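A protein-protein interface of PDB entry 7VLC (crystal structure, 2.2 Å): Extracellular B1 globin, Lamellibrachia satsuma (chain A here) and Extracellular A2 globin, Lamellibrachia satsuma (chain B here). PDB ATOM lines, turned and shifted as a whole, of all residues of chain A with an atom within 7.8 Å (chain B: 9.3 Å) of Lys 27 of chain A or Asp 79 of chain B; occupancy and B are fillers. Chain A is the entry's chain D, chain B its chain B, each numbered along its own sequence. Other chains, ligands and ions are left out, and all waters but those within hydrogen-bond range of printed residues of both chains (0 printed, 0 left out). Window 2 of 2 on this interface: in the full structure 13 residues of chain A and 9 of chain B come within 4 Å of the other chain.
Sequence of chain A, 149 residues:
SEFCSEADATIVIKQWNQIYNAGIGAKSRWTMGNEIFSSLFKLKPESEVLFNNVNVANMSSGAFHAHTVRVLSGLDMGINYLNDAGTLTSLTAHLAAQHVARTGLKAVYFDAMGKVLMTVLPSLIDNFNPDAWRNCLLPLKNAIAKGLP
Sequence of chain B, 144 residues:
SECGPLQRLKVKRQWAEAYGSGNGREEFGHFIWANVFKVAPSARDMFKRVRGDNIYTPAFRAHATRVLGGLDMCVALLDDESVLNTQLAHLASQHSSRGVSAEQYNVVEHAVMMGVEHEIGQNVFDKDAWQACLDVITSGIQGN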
ATOM      1  N   ILE A  24      21.305 -15.247 -19.683  1.00  0.00           N
ATOM      2  CA  ILE A  24      21.770 -16.433 -18.972  1.00  0.00           C
ATOM      3  C   ILE A  24      20.562 -17.293 -18.626  1.00  0.00           C
ATOM      4  O   ILE A  24      19.629 -16.825 -17.958  1.00  0.00           O
ATOM      5  CB  ILE A  24      22.567 -16.065 -17.711  1.00  0.00           C
ATOM      6  CG1 ILE A  24      23.904 -15.437 -18.112  1.00  0.00           C
ATOM      7  CG2 ILE A  24      22.778 -17.285 -16.827  1.00  0.00           C
ATOM      8  CD1 ILE A  24      24.939 -15.445 -17.025  1.00  0.00           C
ATOM      9  N   GLY A  25      20.584 -18.548 -19.076  1.00  0.00           N
ATOM     10  CA  GLY A  25      19.469 -19.440 -18.820  1.00  0.00           C
ATOM     11  C   GLY A  25      19.270 -19.696 -17.338  1.00  0.00           C
ATOM     12  O   GLY A  25      20.218 -19.710 -16.547  1.00  0.00           O
ATOM     13  N   ALA A  26      18.009 -19.912 -16.962  1.00  0.00           N
ATOM     14  CA  ALA A  26      17.660 -20.038 -15.552  1.00  0.00           C
ATOM     15  C   ALA A  26      18.274 -21.267 -14.893  1.00  0.00           C
ATOM     16  O   ALA A  26      18.353 -21.309 -13.661  1.00  0.00           O
ATOM     17  CB  ALA A  26      16.139 -20.068 -15.389  1.00  0.00           C
ATOM     18  N   LYS A  27      18.712 -22.262 -15.671  1.00  0.00           N
ATOM     19  CA  LYS A  27      19.300 -23.456 -15.071  1.00  0.00           C
ATOM     20  C   LYS A  27      20.560 -23.109 -14.285  1.00  0.00           C
ATOM     21  O   LYS A  27      20.734 -23.543 -13.141  1.00  0.00           O
ATOM     22  CB  LYS A  27      19.609 -24.501 -16.144  1.00  0.00           C
ATOM     23  CG  LYS A  27      20.083 -25.830 -15.562  1.00  0.00           C
ATOM     24  CD  LYS A  27      20.747 -26.720 -16.601  1.00  0.00           C
ATOM     25  CE  LYS A  27      19.761 -27.214 -17.646  1.00  0.00           C
ATOM     26  NZ  LYS A  27      20.437 -28.077 -18.654  1.00  0.00           N
ATOM     27  N   SER A  28      21.454 -22.322 -14.883  1.00  0.00           N
ATOM     28  CA  SER A  28      22.622 -21.865 -14.143  1.00  0.00           C
ATOM     29  C   SER A  28      22.254 -20.839 -13.081  1.00  0.00           C
ATOM     30  O   SER A  28      23.014 -20.657 -12.124  1.00  0.00           O
ATOM     31  CB  SER A  28      23.665 -21.292 -15.106  1.00  0.00           C
ATOM     32  OG  SER A  28      23.098 -20.307 -15.948  1.00  0.00           O
ATOM     33  N   ARG A  29      21.101 -20.177 -13.226  1.00  0.00           N
ATOM     34  CA  ARG A  29      20.634 -19.255 -12.195  1.00  0.00           C
ATOM     35  C   ARG A  29      20.361 -19.990 -10.887  1.00  0.00           C
ATOM     36  O   ARG A  29      20.883 -19.611  -9.832  1.00  0.00           O
ATOM     37  CB  ARG A  29      19.379 -18.519 -12.672  1.00  0.00           C
ATOM     38  CG  ARG A  29      19.634 -17.167 -13.328  1.00  0.00           C
ATOM     39  CD  ARG A  29      18.350 -16.626 -13.938  1.00  0.00           C
ATOM     40  NE  ARG A  29      18.315 -15.165 -14.001  1.00  0.00           N
ATOM     41  CZ  ARG A  29      18.721 -14.448 -15.043  1.00  0.00           C
ATOM     42  NH1 ARG A  29      19.202 -15.053 -16.122  1.00  0.00           N
ATOM     43  NH2 ARG A  29      18.642 -13.125 -15.010  1.00  0.00           N
ATOM     44  N   TRP A  30      19.548 -21.052 -10.933  1.00  0.00           N
ATOM     45  CA  TRP A  30      19.259 -21.785  -9.706  1.00  0.00           C
ATOM     46  C   TRP A  30      20.372 -22.752  -9.319  1.00  0.00           C
ATOM     47  O   TRP A  30      20.419 -23.181  -8.160  1.00  0.00           O
ATOM     48  CB  TRP A  30      17.920 -22.532  -9.812  1.00  0.00           C
ATOM     49  CG  TRP A  30      17.840 -23.626 -10.843  1.00  0.00           C
ATOM     50  CD1 TRP A  30      18.583 -24.774 -10.889  1.00  0.00           C
ATOM     51  CD2 TRP A  30      16.928 -23.694 -11.944  1.00  0.00           C
ATOM     52  NE1 TRP A  30      18.205 -25.536 -11.969  1.00  0.00           N
ATOM     53  CE2 TRP A  30      17.189 -24.898 -12.631  1.00  0.00           C
ATOM     54  CE3 TRP A  30      15.922 -22.850 -12.421  1.00  0.00           C
ATOM     55  CZ2 TRP A  30      16.481 -25.275 -13.771  1.00  0.00           C
ATOM     56  CZ3 TRP A  30      15.221 -23.225 -13.552  1.00  0.00           C
ATOM     57  CH2 TRP A  30      15.504 -24.426 -14.216  1.00  0.00           C
ATOM     58  N   THR A  31      21.261 -23.108 -10.253  1.00  0.00           N
ATOM     59  CA  THR A  31      22.466 -23.843  -9.875  1.00  0.00           C
ATOM     60  C   THR A  31      23.309 -23.024  -8.907  1.00  0.00           C
ATOM     61  O   THR A  31      23.783 -23.535  -7.885  1.00  0.00           O
ATOM     62  CB  THR A  31      23.281 -24.212 -11.117  1.00  0.00           C
ATOM     63  OG1 THR A  31      22.507 -25.063 -11.972  1.00  0.00           O
ATOM     64  CG2 THR A  31      24.557 -24.941 -10.722  1.00  0.00           C
ATOM     65  N   MET A  32      23.497 -21.739  -9.209  1.00  0.00           N
ATOM     66  CA  MET A  32      24.174 -20.859  -8.264  1.00  0.00           C
ATOM     67  C   MET A  32      23.341 -20.662  -7.004  1.00  0.00           C
ATOM     68  O   MET A  32      23.886 -20.625  -5.894  1.00  0.00           O
ATOM     69  CB  MET A  32      24.472 -19.512  -8.920  1.00  0.00           C
ATOM     70  CG  MET A  32      25.500 -19.563 -10.037  1.00  0.00           C
ATOM     71  SD  MET A  32      25.597 -17.992 -10.919  1.00  0.00           S
ATOM     72  CE  MET A  32      25.751 -16.850  -9.550  1.00  0.00           C
ATOM     73  N   GLY A  33      22.020 -20.529  -7.160  1.00  0.00           N
ATOM     74  CA  GLY A  33      21.159 -20.376  -5.999  1.00  0.00           C
ATOM     75  C   GLY A  33      21.196 -21.581  -5.078  1.00  0.00           C
ATOM     76  O   GLY A  33      21.262 -21.438  -3.855  1.00  0.00           O
ATOM     77  N   ASN A  34      21.165 -22.786  -5.652  1.00  0.00           N
ATOM     78  CA  ASN A  34      21.207 -23.995  -4.836  1.00  0.00           C
ATOM     79  C   ASN A  34      22.540 -24.121  -4.110  1.00  0.00           C
ATOM     80  O   ASN A  34      22.575 -24.497  -2.932  1.00  0.00           O
ATOM     81  CB  ASN A  34      20.943 -25.234  -5.699  1.00  0.00           C
ATOM     82  CG  ASN A  34      19.461 -25.437  -6.001  1.00  0.00           C
ATOM     83  OD1 ASN A  34      18.592 -25.022  -5.230  1.00  0.00           O
ATOM     84  ND2 ASN A  34      19.169 -26.081  -7.125  1.00  0.00           N
ATOM     85  N   HIS A  65      13.322 -23.269  -6.837  1.00  0.00           N
ATOM     86  CA  HIS A  65      14.068 -22.661  -7.937  1.00  0.00           C
ATOM     87  C   HIS A  65      13.654 -21.211  -8.141  1.00  0.00           C
ATOM     88  O   HIS A  65      14.509 -20.328  -8.291  1.00  0.00           O
ATOM     89  CB  HIS A  65      13.859 -23.456  -9.227  1.00  0.00           C
ATOM     90  CG  HIS A  65      14.707 -24.685  -9.326  1.00  0.00           C
ATOM     91  ND1 HIS A  65      14.557 -25.614 -10.333  1.00  0.00           N
ATOM     92  CD2 HIS A  65      15.714 -25.134  -8.542  1.00  0.00           C
ATOM     93  CE1 HIS A  65      15.438 -26.584 -10.164  1.00  0.00           C
ATOM     94  NE2 HIS A  65      16.152 -26.316  -9.085  1.00  0.00           N
ATOM     95  N   VAL A  69      15.874 -17.758  -7.688  1.00  0.00           N
ATOM     96  CA  VAL A  69      15.903 -16.846  -8.831  1.00  0.00           C
ATOM     97  C   VAL A  69      15.575 -15.427  -8.386  1.00  0.00           C
ATOM     98  O   VAL A  69      16.272 -14.470  -8.742  1.00  0.00           O
ATOM     99  CB  VAL A  69      14.941 -17.333  -9.931  1.00  0.00           C
ATOM    100  CG1 VAL A  69      14.615 -16.204 -10.892  1.00  0.00           C
ATOM    101  CG2 VAL A  69      15.544 -18.514 -10.682  1.00  0.00           C
ATOM    102  N   CYS B   3      34.990 -31.756 -10.100  1.00  0.00           N
ATOM    103  CA  CYS B   3      34.253 -31.042 -11.143  1.00  0.00           C
ATOM    104  C   CYS B   3      32.800 -30.902 -10.695  1.00  0.00           C
ATOM    105  O   CYS B   3      31.898 -31.604 -11.155  1.00  0.00           O
ATOM    106  CB  CYS B   3      34.372 -31.766 -12.479  1.00  0.00           C
ATOM    107  SG  CYS B   3      33.466 -30.989 -13.849  1.00  0.00           S
ATOM    108  N   GLY B   4      32.580 -29.969  -9.772  1.00  0.00           N
ATOM    109  CA  GLY B   4      31.264 -29.727  -9.232  1.00  0.00           C
ATOM    110  C   GLY B   4      30.443 -28.785 -10.090  1.00  0.00           C
ATOM    111  O   GLY B   4      30.857 -28.381 -11.180  1.00  0.00           O
ATOM    112  N   PRO B   5      29.250 -28.417  -9.607  1.00  0.00           N
ATOM    113  CA  PRO B   5      28.393 -27.517 -10.398  1.00  0.00           C
ATOM    114  C   PRO B   5      29.020 -26.156 -10.648  1.00  0.00           C
ATOM    115  O   PRO B   5      28.845 -25.587 -11.734  1.00  0.00           O
ATOM    116  CB  PRO B   5      27.118 -27.410  -9.547  1.00  0.00           C
ATOM    117  CG  PRO B   5      27.142 -28.617  -8.656  1.00  0.00           C
ATOM    118  CD  PRO B   5      28.591 -28.870  -8.371  1.00  0.00           C
ATOM    119  N   LEU B   6      29.752 -25.617  -9.671  1.00  0.00           N
ATOM    120  CA  LEU B   6      30.395 -24.319  -9.852  1.00  0.00           C
ATOM    121  C   LEU B   6      31.538 -24.401 -10.856  1.00  0.00           C
ATOM    122  O   LEU B   6      31.690 -23.513 -11.705  1.00  0.00           O
ATOM    123  CB  LEU B   6      30.900 -23.793  -8.509  1.00  0.00           C
ATOM    124  CG  LEU B   6      29.855 -23.572  -7.412  1.00  0.00           C
ATOM    125  CD1 LEU B   6      30.537 -23.231  -6.095  1.00  0.00           C
ATOM    126  CD2 LEU B   6      28.876 -22.478  -7.808  1.00  0.00           C
ATOM    127  N   GLN B   7      32.358 -25.454 -10.769  1.00  0.00           N
ATOM    128  CA  GLN B   7      33.477 -25.605 -11.694  1.00  0.00           C
ATOM    129  C   GLN B   7      32.998 -25.829 -13.120  1.00  0.00           C
ATOM    130  O   GLN B   7      33.656 -25.388 -14.069  1.00  0.00           O
ATOM    131  CB  GLN B   7      34.382 -26.760 -11.256  1.00  0.00           C
ATOM    132  CG  GLN B   7      35.218 -26.471 -10.011  1.00  0.00           C
ATOM    133  CD  GLN B   7      34.403 -26.499  -8.732  1.00  0.00           C
ATOM    134  OE1 GLN B   7      33.369 -27.161  -8.656  1.00  0.00           O
ATOM    135  NE2 GLN B   7      34.865 -25.776  -7.719  1.00  0.00           N
ATOM    136  N   ARG B   8      31.862 -26.511 -13.289  1.00  0.00           N
ATOM    137  CA  ARG B   8      31.313 -26.705 -14.626  1.00  0.00           C
ATOM    138  C   ARG B   8      30.882 -25.381 -15.244  1.00  0.00           C
ATOM    139  O   ARG B   8      31.093 -25.153 -16.442  1.00  0.00           O
ATOM    140  CB  ARG B   8      30.144 -27.689 -14.569  1.00  0.00           C
ATOM    141  CG  ARG B   8      30.579 -29.118 -14.300  1.00  0.00           C
ATOM    142  CD  ARG B   8      29.463 -29.968 -13.718  1.00  0.00           C
ATOM    143  NE  ARG B   8      29.995 -31.215 -13.176  1.00  0.00           N
ATOM    144  CZ  ARG B   8      29.972 -32.379 -13.814  1.00  0.00           C
ATOM    145  NH1 ARG B   8      29.423 -32.469 -15.019  1.00  0.00           N
ATOM    146  NH2 ARG B   8      30.491 -33.454 -13.241  1.00  0.00           N
ATOM    147  N   LEU B   9      30.287 -24.492 -14.443  1.00  0.00           N
ATOM    148  CA  LEU B   9      29.904 -23.178 -14.953  1.00  0.00           C
ATOM    149  C   LEU B   9      31.129 -22.357 -15.355  1.00  0.00           C
ATOM    150  O   LEU B   9      31.136 -21.731 -16.422  1.00  0.00           O
ATOM    151  CB  LEU B   9      29.073 -22.431 -13.910  1.00  0.00           C
ATOM    152  CG  LEU B   9      27.705 -23.021 -13.549  1.00  0.00           C
ATOM    153  CD1 LEU B   9      27.035 -22.190 -12.466  1.00  0.00           C
ATOM    154  CD2 LEU B   9      26.811 -23.116 -14.774  1.00  0.00           C
ATOM    155  N   LYS B  10      32.170 -22.349 -14.515  1.00  0.00           N
ATOM    156  CA  LYS B  10      33.383 -21.597 -14.835  1.00  0.00           C
ATOM    157  C   LYS B  10      34.052 -22.128 -16.097  1.00  0.00           C
ATOM    158  O   LYS B  10      34.459 -21.347 -16.966  1.00  0.00           O
ATOM    159  CB  LYS B  10      34.357 -21.646 -13.656  1.00  0.00           C
ATOM    160  CG  LYS B  10      35.732 -21.079 -13.965  1.00  0.00           C
ATOM    161  CD  LYS B  10      35.857 -19.622 -13.540  1.00  0.00           C
ATOM    162  CE  LYS B  10      36.364 -19.511 -12.109  1.00  0.00           C
ATOM    163  NZ  LYS B  10      36.827 -18.135 -11.763  1.00  0.00           N
ATOM    164  N   VAL B  11      34.175 -23.453 -16.215  1.00  0.00           N
ATOM    165  CA  VAL B  11      34.779 -24.050 -17.404  1.00  0.00           C
ATOM    166  C   VAL B  11      33.968 -23.711 -18.648  1.00  0.00           C
ATOM    167  O   VAL B  11      34.531 -23.453 -19.720  1.00  0.00           O
ATOM    168  CB  VAL B  11      34.934 -25.574 -17.221  1.00  0.00           C
ATOM    169  CG1 VAL B  11      35.237 -26.251 -18.555  1.00  0.00           C
ATOM    170  CG2 VAL B  11      36.040 -25.873 -16.223  1.00  0.00           C
ATOM    171  N   LYS B  12      32.635 -23.705 -18.526  1.00  0.00           N
ATOM    172  CA  LYS B  12      31.781 -23.342 -19.654  1.00  0.00           C
ATOM    173  C   LYS B  12      32.119 -21.952 -20.180  1.00  0.00           C
ATOM    174  O   LYS B  12      32.399 -21.775 -21.373  1.00  0.00           O
ATOM    175  CB  LYS B  12      30.309 -23.412 -19.241  1.00  0.00           C
ATOM    176  CG  LYS B  12      29.691 -24.807 -19.277  1.00  0.00           C
ATOM    177  CD  LYS B  12      28.321 -24.807 -18.618  1.00  0.00           C
ATOM    178  CE  LYS B  12      27.583 -26.107 -18.856  1.00  0.00           C
ATOM    179  NZ  LYS B  12      27.045 -26.184 -20.240  1.00  0.00           N
ATOM    180  N   ASP B  72      33.543 -28.964 -27.473  1.00  0.00           N
ATOM    181  CA  ASP B  72      32.478 -27.980 -27.297  1.00  0.00           C
ATOM    182  C   ASP B  72      31.166 -28.652 -26.912  1.00  0.00           C
ATOM    183  O   ASP B  72      30.434 -28.151 -26.050  1.00  0.00           O
ATOM    184  CB  ASP B  72      32.299 -27.160 -28.575  1.00  0.00           C
ATOM    185  CG  ASP B  72      31.235 -26.087 -28.434  1.00  0.00           C
ATOM    186  OD1 ASP B  72      31.521 -25.052 -27.797  1.00  0.00           O
ATOM    187  OD2 ASP B  72      30.114 -26.276 -28.945  1.00  0.00           O
ATOM    188  N   MET B  73      30.856 -29.791 -27.539  1.00  0.00           N
ATOM    189  CA  MET B  73      29.648 -30.525 -27.179  1.00  0.00           C
ATOM    190  C   MET B  73      29.711 -31.020 -25.741  1.00  0.00           C
ATOM    191  O   MET B  73      28.724 -30.927 -25.003  1.00  0.00           O
ATOM    192  CB  MET B  73      29.436 -31.691 -28.142  1.00  0.00           C
ATOM    193  CG  MET B  73      29.063 -31.268 -29.546  1.00  0.00           C
ATOM    194  SD  MET B  73      28.633 -32.670 -30.594  1.00  0.00           S
ATOM    195  CE  MET B  73      30.242 -33.415 -30.851  1.00  0.00           C
ATOM    196  N   CYS B  74      30.867 -31.534 -25.317  1.00  0.00           N
ATOM    197  CA  CYS B  74      31.005 -32.014 -23.944  1.00  0.00           C
ATOM    198  C   CYS B  74      30.910 -30.871 -22.941  1.00  0.00           C
ATOM    199  O   CYS B  74      30.201 -30.976 -21.934  1.00  0.00           O
ATOM    200  CB  CYS B  74      32.328 -32.763 -23.771  1.00  0.00           C
ATOM    201  SG  CYS B  74      32.478 -34.244 -24.780  1.00  0.00           S
ATOM    202  N   VAL B  75      31.630 -29.771 -23.191  1.00  0.00           N
ATOM    203  CA  VAL B  75      31.606 -28.641 -22.264  1.00  0.00           C
ATOM    204  C   VAL B  75      30.199 -28.061 -22.163  1.00  0.00           C
ATOM    205  O   VAL B  75      29.714 -27.751 -21.067  1.00  0.00           O
ATOM    206  CB  VAL B  75      32.634 -27.576 -22.692  1.00  0.00           C
ATOM    207  CG1 VAL B  75      32.495 -26.325 -21.840  1.00  0.00           C
ATOM    208  CG2 VAL B  75      34.052 -28.134 -22.590  1.00  0.00           C
ATOM    209  N   ALA B  76      29.512 -27.924 -23.298  1.00  0.00           N
ATOM    210  CA  ALA B  76      28.137 -27.441 -23.292  1.00  0.00           C
ATOM    211  C   ALA B  76      27.179 -28.393 -22.587  1.00  0.00           C
ATOM    212  O   ALA B  76      26.060 -27.984 -22.261  1.00  0.00           O
ATOM    213  CB  ALA B  76      27.659 -27.199 -24.724  1.00  0.00           C
ATOM    214  N   LEU B  77      27.586 -29.639 -22.341  1.00  0.00           N
ATOM    215  CA  LEU B  77      26.743 -30.633 -21.690  1.00  0.00           C
ATOM    216  C   LEU B  77      27.180 -30.940 -20.263  1.00  0.00           C
ATOM    217  O   LEU B  77      26.614 -31.842 -19.636  1.00  0.00           O
ATOM    218  CB  LEU B  77      26.717 -31.922 -22.513  1.00  0.00           C
ATOM    219  CG  LEU B  77      25.826 -31.897 -23.751  1.00  0.00           C
ATOM    220  CD1 LEU B  77      26.034 -33.154 -24.576  1.00  0.00           C
ATOM    221  CD2 LEU B  77      24.375 -31.761 -23.334  1.00  0.00           C
ATOM    222  N   LEU B  78      28.169 -30.216 -19.731  1.00  0.00           N
ATOM    223  CA  LEU B  78      28.657 -30.502 -18.384  1.00  0.00           C
ATOM    224  C   LEU B  78      27.580 -30.312 -17.324  1.00  0.00           C
ATOM    225  O   LEU B  78      27.674 -30.911 -16.247  1.00  0.00           O
ATOM    226  CB  LEU B  78      29.864 -29.623 -18.055  1.00  0.00           C
ATOM    227  CG  LEU B  78      31.165 -29.945 -18.797  1.00  0.00           C
ATOM    228  CD1 LEU B  78      32.309 -29.053 -18.312  1.00  0.00           C
ATOM    229  CD2 LEU B  78      31.519 -31.414 -18.643  1.00  0.00           C
ATOM    230  N   ASP B  79      26.563 -29.499 -17.599  1.00  0.00           N
ATOM    231  CA  ASP B  79      25.456 -29.290 -16.677  1.00  0.00           C
ATOM    232  C   ASP B  79      24.267 -30.190 -16.982  1.00  0.00           C
ATOM    233  O   ASP B  79      23.187 -29.984 -16.421  1.00  0.00           O
ATOM    234  CB  ASP B  79      25.019 -27.825 -16.705  1.00  0.00           C
ATOM    235  CG  ASP B  79      24.472 -27.410 -18.053  1.00  0.00           C
ATOM    236  OD1 ASP B  79      24.951 -27.938 -19.078  1.00  0.00           O
ATOM    237  OD2 ASP B  79      23.562 -26.558 -18.089  1.00  0.00           O
ATOM    238  N   ASP B  80      24.440 -31.178 -17.865  1.00  0.00           N
ATOM    239  CA  ASP B  80      23.370 -32.093 -18.273  1.00  0.00           C
ATOM    240  C   ASP B  80      23.949 -33.506 -18.217  1.00  0.00           C
ATOM    241  O   ASP B  80      24.396 -34.045 -19.231  1.00  0.00           O
ATOM    242  CB  ASP B  80      22.844 -31.737 -19.664  1.00  0.00           C
ATOM    243  CG  ASP B  80      21.471 -32.319 -19.941  1.00  0.00           C
ATOM    244  OD1 ASP B  80      21.110 -33.336 -19.313  1.00  0.00           O
ATOM    245  OD2 ASP B  80      20.751 -31.754 -20.790  1.00  0.00           O
ATOM    246  N   GLU B  81      23.923 -34.101 -17.021  1.00  0.00           N
ATOM    247  CA  GLU B  81      24.626 -35.359 -16.784  1.00  0.00           C
ATOM    248  C   GLU B  81      24.159 -36.460 -17.730  1.00  0.00           C
ATOM    249  O   GLU B  81      24.981 -37.200 -18.284  1.00  0.00           O
ATOM    250  CB  GLU B  81      24.438 -35.787 -15.327  1.00  0.00           C
ATOM    251  CG  GLU B  81      25.145 -37.078 -14.946  1.00  0.00           C
ATOM    252  CD  GLU B  81      26.654 -36.931 -14.904  1.00  0.00           C
ATOM    253  OE1 GLU B  81      27.142 -35.780 -14.928  1.00  0.00           O
ATOM    254  OE2 GLU B  81      27.352 -37.966 -14.847  1.00  0.00           O
ATOM    255  N   SER B  82      22.846 -36.579 -17.935  1.00  0.00           N
ATOM    256  CA  SER B  82      22.318 -37.665 -18.756  1.00  0.00           C
ATOM    257  C   SER B  82      22.785 -37.547 -20.202  1.00  0.00           C
ATOM    258  O   SER B  82      23.317 -38.504 -20.774  1.00  0.00           O
ATOM    259  CB  SER B  82      20.790 -37.678 -18.681  1.00  0.00           C
ATOM    260  OG  SER B  82      20.244 -38.625 -19.582  1.00  0.00           O
ATOM    261  N   VAL B  83      22.596 -36.373 -20.811  1.00  0.00           N
ATOM    262  CA  VAL B  83      22.963 -36.195 -22.213  1.00  0.00           C
ATOM    263  C   VAL B  83      24.478 -36.209 -22.385  1.00  0.00           C
ATOM    264  O   VAL B  83      24.988 -36.676 -23.413  1.00  0.00           O
ATOM    265  CB  VAL B  83      22.340 -34.896 -22.760  1.00  0.00           C
ATOM    266  CG1 VAL B  83      22.483 -34.830 -24.273  1.00  0.00           C
ATOM    267  CG2 VAL B  83      20.874 -34.792 -22.353  1.00  0.00           C
ATOM    268  N   LEU B  84      25.222 -35.710 -21.392  1.00  0.00           N
ATOM    269  CA  LEU B  84      26.680 -35.712 -21.476  1.00  0.00           C
ATOM    270  C   LEU B  84      27.229 -37.129 -21.568  1.00  0.00           C
ATOM    271  O   LEU B  84      28.143 -37.397 -22.357  1.00  0.00           O
ATOM    272  CB  LEU B  84      27.278 -34.993 -20.265  1.00  0.00           C
ATOM    273  CG  LEU B  84      28.789 -35.128 -20.054  1.00  0.00           C
ATOM    274  CD1 LEU B  84      29.575 -34.471 -21.185  1.00  0.00           C
ATOM    275  CD2 LEU B  84      29.191 -34.540 -18.718  1.00  0.00           C
ATOM    276  N   ASN B  85      26.687 -38.049 -20.764  1.00  0.00           N
ATOM    277  CA  ASN B  85      27.157 -39.431 -20.802  1.00  0.00           C
ATOM    278  C   ASN B  85      26.878 -40.071 -22.156  1.00  0.00           C
ATOM    279  O   ASN B  85      27.686 -40.865 -22.652  1.00  0.00           O
ATOM    280  CB  ASN B  85      26.506 -40.240 -19.681  1.00  0.00           C
ATOM    281  CG  ASN B  85      26.947 -39.782 -18.308  1.00  0.00           C
ATOM    282  OD1 ASN B  85      28.110 -39.438 -18.102  1.00  0.00           O
ATOM    283  ND2 ASN B  85      26.014 -39.765 -17.358  1.00  0.00           N
ATOM    284  N   CYS B 133      37.337 -31.124 -14.621  1.00  0.00           N
ATOM    285  CA  CYS B 133      36.246 -31.340 -15.565  1.00  0.00           C
ATOM    286  C   CYS B 133      36.704 -31.976 -16.871  1.00  0.00           C
ATOM    287  O   CYS B 133      35.912 -32.667 -17.522  1.00  0.00           O
ATOM    288  CB  CYS B 133      35.524 -30.018 -15.844  1.00  0.00           C
ATOM    289  SG  CYS B 133      34.620 -29.406 -14.416  1.00  0.00           S
ATOM    290  N   VAL B 136      36.734 -35.657 -16.126  1.00  0.00           N
ATOM    291  CA  VAL B 136      35.399 -36.225 -16.302  1.00  0.00           C
ATOM    292  C   VAL B 136      35.129 -36.521 -17.773  1.00  0.00           C
ATOM    293  O   VAL B 136      34.490 -37.527 -18.112  1.00  0.00           O
ATOM    294  CB  VAL B 136      34.338 -35.277 -15.709  1.00  0.00           C
ATOM    295  CG1 VAL B 136      32.937 -35.793 -15.986  1.00  0.00           C
ATOM    296  CG2 VAL B 136      34.554 -35.103 -14.215  1.00  0.00           C
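The side-chain carboxylate of Asp 79 of chain B lies within salt-bridge range of the side-chain amino group of Lys 27 of chain A (3.5 Å).
NZ of Lys 12 of chain B lies within salt-bridge range of OD1 of Asp 79 of chain B (3.0 Å).
The backbone carbonyl oxygen of Gly 25 of chain A is in hydrogen-bond range of the side-chain hydroxyl of Ser 28 of chain A (3.0 Å).
The backbone carbonyl oxygen (O) of Lys 27 of chain A lies close to the indole nitrogen (NE1) of Trp 30 of chain A, at 3.4 Å.
O of Lys 27 of chain A is in hydrogen-bond range of OG1 of Thr 31 of chain A, 2.6 Å away.
SG of Cys 133 of chain B forms a disulfide with SG of Cys 3 of chain B (2.0 Å).
Among the printed residues, merely in contact across the chains: Ser 28 of chain A with Leu 9 of chain B (3.7 Å), Thr 31 of chain A with Pro 5 of chain B (3.7 Å) and Met 32 of chain A with Leu 9 of chain B (3.9 Å).
No residue of chain B comes within 4 Å of Ala 26 of chain A.
Printed residues of chain B within 4 Å of Lys 27 of chain A: Asp 79.
Ser 28 of chain A touches just one residue of chain B: Leu 9.
No residue of chain B comes within 4 Å of Trp 30 of chain A.
Printed residues of chain B within 4 Å of Met 32 of chain A: Leu 9 (3.9 Å).
Gly 4 of chain B touches none of the printed residues of chain A.
Of the printed residues of chain A, Pro 5 of chain B touches Thr 31 (3.7 Å).
Of chain A, only Lys 27 comes within 4 Å of Asp 79 of chain B.
The nearest printed residue of chain B that does not touch Met 32 of chain A is Leu 6 of chain B (5.0 Å).
Of the 26 printed residues of chain B, 3 touch a printed residue of chain A.
Hydrophobic or aromatic side chains of chain B within 4 Å of the printed part of chain A: Pro 5 and Leu 9.
Of the 13 printed residues of chain A, 4 touch a printed residue of chain B.
Hydrophobic or aromatic side chains of chain A within 4 Å of the printed part of chain B: Met 32.
Among the printed residues, Asp or Glu carboxylates within 4 Å of a Lys or Arg side-chain nitrogen of the other chain: Lys 27 of chain A with Asp 79 of chain B (3.5 Å).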
